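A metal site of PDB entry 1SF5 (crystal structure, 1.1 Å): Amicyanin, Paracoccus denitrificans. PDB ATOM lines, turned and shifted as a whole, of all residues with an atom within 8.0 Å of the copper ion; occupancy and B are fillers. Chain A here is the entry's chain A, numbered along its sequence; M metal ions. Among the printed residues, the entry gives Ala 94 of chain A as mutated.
The backbone carbonyl oxygen (O) of Met 98 lies within hydrogen-bond range of the backbone NH (N) of Cys 92 (3.1 Å).
The side-chain sulfur (SG) of Cys 92 sits close to the backbone NH (N) of Asn 54 (3.7 Å).
OH of Tyr 30 sits at hydrogen-bond distance from N of Cys 92.
ND1 of His 53 lies close to SD of Met 98 (3.4 Å).
A ring nitrogen (NE2) of His 53 sits close to the side-chain sulfur (SD) of Met 28, at 3.8 Å.
A ring nitrogen (NE2) of His 53 lies within hydrogen-bond range of the side-chain carboxylate of Glu 49 (2.7 Å).
N of Met 72 lies within hydrogen-bond range of O of His 53 (2.7 Å).
OD1 of MHO 51 lies within hydrogen-bond range of a ring nitrogen (NE2) of His 95, 2.6 Å away.
Merely in contact with the copper ion: Met 98 and Pro 52.
Of the 21 residues printed, 5 come within 4 Å of the copper ion.
The nearest printed residue that does not touch the copper ion is Asn 54 (4.6 Å).
The copper ion is bound by SG of Cys 92, ND1 of His 53 and ND1 of His 95.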
ATOM      1  N   ILE A  25     -26.060 -16.695  -5.490  1.00  0.00           N
ATOM      2  CA  ILE A  25     -26.268 -15.264  -5.377  1.00  0.00           C
ATOM      3  C   ILE A  25     -27.165 -14.900  -6.553  1.00  0.00           C
ATOM      4  O   ILE A  25     -26.758 -15.008  -7.723  1.00  0.00           O
ATOM      5  CB  ILE A  25     -24.963 -14.465  -5.373  1.00  0.00           C
ATOM      6  CG1 ILE A  25     -23.909 -15.076  -4.430  1.00  0.00           C
ATOM      7  CG2 ILE A  25     -25.286 -13.009  -5.073  1.00  0.00           C
ATOM      8  CD1 ILE A  25     -22.568 -14.420  -4.503  1.00  0.00           C
ATOM      9  N   MET A  28     -30.153 -10.313  -6.105  1.00  0.00           N
ATOM     10  CA  MET A  28     -29.454  -9.382  -5.229  1.00  0.00           C
ATOM     11  C   MET A  28     -29.441  -9.815  -3.767  1.00  0.00           C
ATOM     12  O   MET A  28     -29.482  -8.993  -2.855  1.00  0.00           O
ATOM     13  CB  MET A  28     -29.951  -7.930  -5.360  1.00  0.00           C
ATOM     14  CG  MET A  28     -29.495  -7.301  -6.666  1.00  0.00           C
ATOM     15  SD  MET A  28     -27.805  -6.941  -7.115  1.00  0.00           S
ATOM     16  CE  MET A  28     -27.262  -6.016  -5.692  1.00  0.00           C
ATOM     17  N   LYS A  29     -29.399 -11.125  -3.540  1.00  0.00           N
ATOM     18  CA  LYS A  29     -29.339 -11.690  -2.215  1.00  0.00           C
ATOM     19  C   LYS A  29     -28.482 -12.939  -2.233  1.00  0.00           C
ATOM     20  O   LYS A  29     -28.354 -13.642  -3.246  1.00  0.00           O
ATOM     21  CB  LYS A  29     -30.733 -12.095  -1.731  1.00  0.00           C
ATOM     22  CG  LYS A  29     -31.716 -10.958  -1.666  1.00  0.00           C
ATOM     23  CD  LYS A  29     -33.148 -11.427  -1.475  1.00  0.00           C
ATOM     24  CE  LYS A  29     -33.898 -11.547  -2.772  1.00  0.00           C
ATOM     25  NZ  LYS A  29     -35.199 -10.888  -2.881  1.00  0.00           N
ATOM     26  N   TYR A  30     -27.899 -13.242  -1.073  1.00  0.00           N
ATOM     27  CA  TYR A  30     -27.367 -14.575  -0.834  1.00  0.00           C
ATOM     28  C   TYR A  30     -28.571 -15.477  -0.577  1.00  0.00           C
ATOM     29  O   TYR A  30     -29.308 -15.289   0.387  1.00  0.00           O
ATOM     30  CB  TYR A  30     -26.433 -14.581   0.319  1.00  0.00           C
ATOM     31  CG  TYR A  30     -25.242 -13.665   0.189  1.00  0.00           C
ATOM     32  CD1 TYR A  30     -24.245 -13.904  -0.732  1.00  0.00           C
ATOM     33  CD2 TYR A  30     -25.086 -12.536   1.000  1.00  0.00           C
ATOM     34  CE1 TYR A  30     -23.145 -13.086  -0.874  1.00  0.00           C
ATOM     35  CE2 TYR A  30     -23.990 -11.715   0.903  1.00  0.00           C
ATOM     36  CZ  TYR A  30     -23.008 -12.002  -0.061  1.00  0.00           C
ATOM     37  OH  TYR A  30     -21.933 -11.151  -0.079  1.00  0.00           O
ATOM     38  N   ASN A  47     -22.244 -16.699  -8.365  1.00  0.00           N
ATOM     39  CA  ASN A  47     -22.925 -15.499  -8.797  1.00  0.00           C
ATOM     40  C   ASN A  47     -23.750 -15.781 -10.059  1.00  0.00           C
ATOM     41  O   ASN A  47     -23.193 -16.190 -11.080  1.00  0.00           O
ATOM     42  CB  ASN A  47     -21.982 -14.322  -9.106  1.00  0.00           C
ATOM     43  CG  ASN A  47     -22.730 -13.030  -9.408  1.00  0.00           C
ATOM     44  OD1 ASN A  47     -23.961 -12.976  -9.210  1.00  0.00           O
ATOM     45  ND2 ASN A  47     -22.016 -12.025  -9.850  1.00  0.00           N
ATOM     46  N   GLU A  49     -25.934 -13.375 -11.351  1.00  0.00           N
ATOM     47  CA  GLU A  49     -26.295 -12.120 -11.922  1.00  0.00           C
ATOM     48  C   GLU A  49     -25.210 -11.337 -12.652  1.00  0.00           C
ATOM     49  O   GLU A  49     -24.059 -11.588 -12.446  1.00  0.00           O
ATOM     50  CB  GLU A  49     -26.727 -11.163 -10.784  1.00  0.00           C
ATOM     51  CG  GLU A  49     -27.470 -11.791  -9.643  1.00  0.00           C
ATOM     52  CD  GLU A  49     -28.253 -10.745  -8.860  1.00  0.00           C
ATOM     53  OE1 GLU A  49     -29.465 -10.563  -8.998  1.00  0.00           O
ATOM     54  OE2 GLU A  49     -27.598 -10.074  -8.069  1.00  0.00           O
ATOM     55  N   MHO A  51     -24.547  -8.200 -12.233  1.00  0.00           N
ATOM     56  CA  MHO A  51     -23.806  -7.349 -11.316  1.00  0.00           C
ATOM     57  CB  MHO A  51     -24.771  -6.769 -10.328  1.00  0.00           C
ATOM     58  CG  MHO A  51     -24.126  -5.888  -9.288  1.00  0.00           C
ATOM     59  SD  MHO A  51     -23.320  -4.449  -9.939  1.00  0.00           S
ATOM     60  CE  MHO A  51     -24.731  -3.688 -10.716  1.00  0.00           C
ATOM     61  C   MHO A  51     -22.780  -8.204 -10.583  1.00  0.00           C
ATOM     62  O   MHO A  51     -23.138  -9.256 -10.052  1.00  0.00           O
ATOM     63  OD1 MHO A  51     -23.027  -3.331  -8.583  1.00  0.00           O
ATOM     64  N   PRO A  52     -21.531  -7.783 -10.489  1.00  0.00           N
ATOM     65  CA  PRO A  52     -20.551  -8.568  -9.724  1.00  0.00           C
ATOM     66  C   PRO A  52     -20.877  -8.575  -8.244  1.00  0.00           C
ATOM     67  O   PRO A  52     -21.411  -7.577  -7.746  1.00  0.00           O
ATOM     68  CB  PRO A  52     -19.238  -7.813 -10.004  1.00  0.00           C
ATOM     69  CG  PRO A  52     -19.485  -7.060 -11.266  1.00  0.00           C
ATOM     70  CD  PRO A  52     -20.911  -6.584 -11.139  1.00  0.00           C
ATOM     71  N   HIS A  53     -20.496  -9.653  -7.569  1.00  0.00           N
ATOM     72  CA  HIS A  53     -20.651  -9.812  -6.137  1.00  0.00           C
ATOM     73  C   HIS A  53     -19.416 -10.529  -5.538  1.00  0.00           C
ATOM     74  O   HIS A  53     -18.772 -11.301  -6.240  1.00  0.00           O
ATOM     75  CB  HIS A  53     -21.872 -10.606  -5.786  1.00  0.00           C
ATOM     76  CG  HIS A  53     -23.178 -10.030  -6.174  1.00  0.00           C
ATOM     77  ND1 HIS A  53     -23.729  -8.910  -5.610  1.00  0.00           N
ATOM     78  CD2 HIS A  53     -24.046 -10.443  -7.133  1.00  0.00           C
ATOM     79  CE1 HIS A  53     -24.875  -8.697  -6.185  1.00  0.00           C
ATOM     80  NE2 HIS A  53     -25.126  -9.613  -7.119  1.00  0.00           N
ATOM     81  N   ASN A  54     -19.200 -10.285  -4.251  1.00  0.00           N
ATOM     82  CA  ASN A  54     -18.187 -11.064  -3.527  1.00  0.00           C
ATOM     83  C   ASN A  54     -18.782 -11.506  -2.191  1.00  0.00           C
ATOM     84  O   ASN A  54     -19.954 -11.305  -1.904  1.00  0.00           O
ATOM     85  CB  ASN A  54     -16.896 -10.276  -3.375  1.00  0.00           C
ATOM     86  CG  ASN A  54     -16.940  -9.202  -2.325  1.00  0.00           C
ATOM     87  OD1 ASN A  54     -18.011  -8.744  -1.931  1.00  0.00           O
ATOM     88  ND2 ASN A  54     -15.777  -8.771  -1.863  1.00  0.00           N
ATOM     89  N   VAL A  55     -17.911 -12.044  -1.347  1.00  0.00           N
ATOM     90  CA  VAL A  55     -18.151 -12.247   0.054  1.00  0.00           C
ATOM     91  C   VAL A  55     -17.002 -11.603   0.811  1.00  0.00           C
ATOM     92  O   VAL A  55     -15.838 -11.706   0.415  1.00  0.00           O
ATOM     93  CB  VAL A  55     -18.321 -13.730   0.455  1.00  0.00           C
ATOM     94  CG1 VAL A  55     -19.561 -14.291  -0.197  1.00  0.00           C
ATOM     95  CG2 VAL A  55     -17.080 -14.574   0.128  1.00  0.00           C
ATOM     96  N   MET A  71     -14.288 -10.305  -6.626  1.00  0.00           N
ATOM     97  CA  MET A  71     -15.541 -10.097  -7.291  1.00  0.00           C
ATOM     98  C   MET A  71     -15.800 -11.214  -8.317  1.00  0.00           C
ATOM     99  O   MET A  71     -14.953 -11.478  -9.184  1.00  0.00           O
ATOM    100  CB  MET A  71     -15.567  -8.767  -8.048  1.00  0.00           C
ATOM    101  CG  MET A  71     -15.231  -7.575  -7.230  1.00  0.00           C
ATOM    102  SD  MET A  71     -16.191  -7.350  -5.722  1.00  0.00           S
ATOM    103  CE  MET A  71     -17.738  -7.723  -6.290  1.00  0.00           C
ATOM    104  N   MET A  72     -16.917 -11.877  -8.182  1.00  0.00           N
ATOM    105  CA  MET A  72     -17.362 -12.926  -9.089  1.00  0.00           C
ATOM    106  C   MET A  72     -18.199 -12.283 -10.192  1.00  0.00           C
ATOM    107  O   MET A  72     -19.168 -11.604  -9.885  1.00  0.00           O
ATOM    108  CB  MET A  72     -18.239 -13.980  -8.383  1.00  0.00           C
ATOM    109  CG  MET A  72     -17.543 -14.896  -7.426  1.00  0.00           C
ATOM    110  SD  MET A  72     -18.645 -15.847  -6.356  1.00  0.00           S
ATOM    111  CE  MET A  72     -18.777 -14.603  -5.086  1.00  0.00           C
ATOM    112  N   HIS A  91     -20.651  -9.968   4.199  1.00  0.00           N
ATOM    113  CA  HIS A  91     -21.437  -9.087   3.368  1.00  0.00           C
ATOM    114  C   HIS A  91     -20.782  -8.962   2.020  1.00  0.00           C
ATOM    115  O   HIS A  91     -19.648  -9.385   1.785  1.00  0.00           O
ATOM    116  CB  HIS A  91     -21.591  -7.701   4.043  1.00  0.00           C
ATOM    117  CG  HIS A  91     -20.336  -6.898   4.159  1.00  0.00           C
ATOM    118  ND1 HIS A  91     -19.357  -7.116   5.072  1.00  0.00           N
ATOM    119  CD2 HIS A  91     -19.864  -5.906   3.359  1.00  0.00           C
ATOM    120  CE1 HIS A  91     -18.349  -6.285   4.914  1.00  0.00           C
ATOM    121  NE2 HIS A  91     -18.628  -5.541   3.856  1.00  0.00           N
ATOM    122  N   CYS A  92     -21.476  -8.286   1.107  1.00  0.00           N
ATOM    123  CA  CYS A  92     -20.888  -7.920  -0.198  1.00  0.00           C
ATOM    124  C   CYS A  92     -20.238  -6.558  -0.148  1.00  0.00           C
ATOM    125  O   CYS A  92     -20.865  -5.592   0.280  1.00  0.00           O
ATOM    126  CB  CYS A  92     -21.970  -7.943  -1.254  1.00  0.00           C
ATOM    127  SG  CYS A  92     -21.355  -7.651  -2.922  1.00  0.00           S
ATOM    128  N   THR A  93     -18.947  -6.452  -0.526  1.00  0.00           N
ATOM    129  CA  THR A  93     -18.230  -5.224  -0.394  1.00  0.00           C
ATOM    130  C   THR A  93     -18.906  -4.072  -1.134  1.00  0.00           C
ATOM    131  O   THR A  93     -18.990  -2.960  -0.638  1.00  0.00           O
ATOM    132  CB  THR A  93     -16.801  -5.381  -0.914  1.00  0.00           C
ATOM    133  OG1 THR A  93     -16.166  -6.473  -0.257  1.00  0.00           O
ATOM    134  CG2 THR A  93     -16.001  -4.092  -0.699  1.00  0.00           C
ATOM    135  N   ALA A  94     -19.369  -4.387  -2.355  1.00  0.00           N
ATOM    136  CA  ALA A  94     -19.959  -3.403  -3.237  1.00  0.00           C
ATOM    137  C   ALA A  94     -21.373  -3.024  -2.814  1.00  0.00           C
ATOM    138  O   ALA A  94     -21.818  -1.899  -3.071  1.00  0.00           O
ATOM    139  CB  ALA A  94     -19.976  -3.948  -4.651  1.00  0.00           C
ATOM    140  N   HIS A  95     -22.060  -4.040  -2.234  1.00  0.00           N
ATOM    141  CA  HIS A  95     -23.454  -3.939  -1.861  1.00  0.00           C
ATOM    142  C   HIS A  95     -23.674  -4.346  -0.398  1.00  0.00           C
ATOM    143  O   HIS A  95     -24.158  -5.481  -0.158  1.00  0.00           O
ATOM    144  CB  HIS A  95     -24.329  -4.864  -2.712  1.00  0.00           C
ATOM    145  CG  HIS A  95     -24.032  -4.692  -4.183  1.00  0.00           C
ATOM    146  ND1 HIS A  95     -23.437  -5.721  -4.925  1.00  0.00           N
ATOM    147  CD2 HIS A  95     -24.288  -3.684  -5.021  1.00  0.00           C
ATOM    148  CE1 HIS A  95     -23.341  -5.261  -6.155  1.00  0.00           C
ATOM    149  NE2 HIS A  95     -23.833  -4.020  -6.239  1.00  0.00           N
ATOM    150  N   PRO A  96     -23.264  -3.539   0.553  1.00  0.00           N
ATOM    151  CA  PRO A  96     -23.243  -3.995   1.960  1.00  0.00           C
ATOM    152  C   PRO A  96     -24.618  -4.289   2.538  1.00  0.00           C
ATOM    153  O   PRO A  96     -24.667  -4.923   3.601  1.00  0.00           O
ATOM    154  CB  PRO A  96     -22.474  -2.890   2.674  1.00  0.00           C
ATOM    155  CG  PRO A  96     -22.613  -1.725   1.798  1.00  0.00           C
ATOM    156  CD  PRO A  96     -22.637  -2.205   0.381  1.00  0.00           C
ATOM    157  N   PHE A  97     -25.697  -3.943   1.859  1.00  0.00           N
ATOM    158  CA  PHE A  97     -26.985  -4.404   2.328  1.00  0.00           C
ATOM    159  C   PHE A  97     -27.125  -5.907   2.127  1.00  0.00           C
ATOM    160  O   PHE A  97     -28.079  -6.439   2.729  1.00  0.00           O
ATOM    161  CB  PHE A  97     -28.135  -3.698   1.604  1.00  0.00           C
ATOM    162  CG  PHE A  97     -27.957  -3.671   0.111  1.00  0.00           C
ATOM    163  CD1 PHE A  97     -28.443  -4.699  -0.676  1.00  0.00           C
ATOM    164  CD2 PHE A  97     -27.311  -2.612  -0.515  1.00  0.00           C
ATOM    165  CE1 PHE A  97     -28.275  -4.637  -2.054  1.00  0.00           C
ATOM    166  CE2 PHE A  97     -27.145  -2.563  -1.899  1.00  0.00           C
ATOM    167  CZ  PHE A  97     -27.644  -3.584  -2.695  1.00  0.00           C
ATOM    168  N   MET A  98     -26.305  -6.545   1.365  1.00  0.00           N
ATOM    169  CA  MET A  98     -26.346  -8.018   1.221  1.00  0.00           C
ATOM    170  C   MET A  98     -25.543  -8.655   2.339  1.00  0.00           C
ATOM    171  O   MET A  98     -24.320  -8.467   2.350  1.00  0.00           O
ATOM    172  CB  MET A  98     -25.712  -8.427  -0.085  1.00  0.00           C
ATOM    173  CG  MET A  98     -26.436  -7.963  -1.314  1.00  0.00           C
ATOM    174  SD  MET A  98     -25.623  -8.316  -2.869  1.00  0.00           S
ATOM    175  CE  MET A  98     -25.710 -10.083  -2.785  1.00  0.00           C
HETATM  176 CU    CU M   1     -22.893  -7.608  -4.268  1.00  0.00          CU
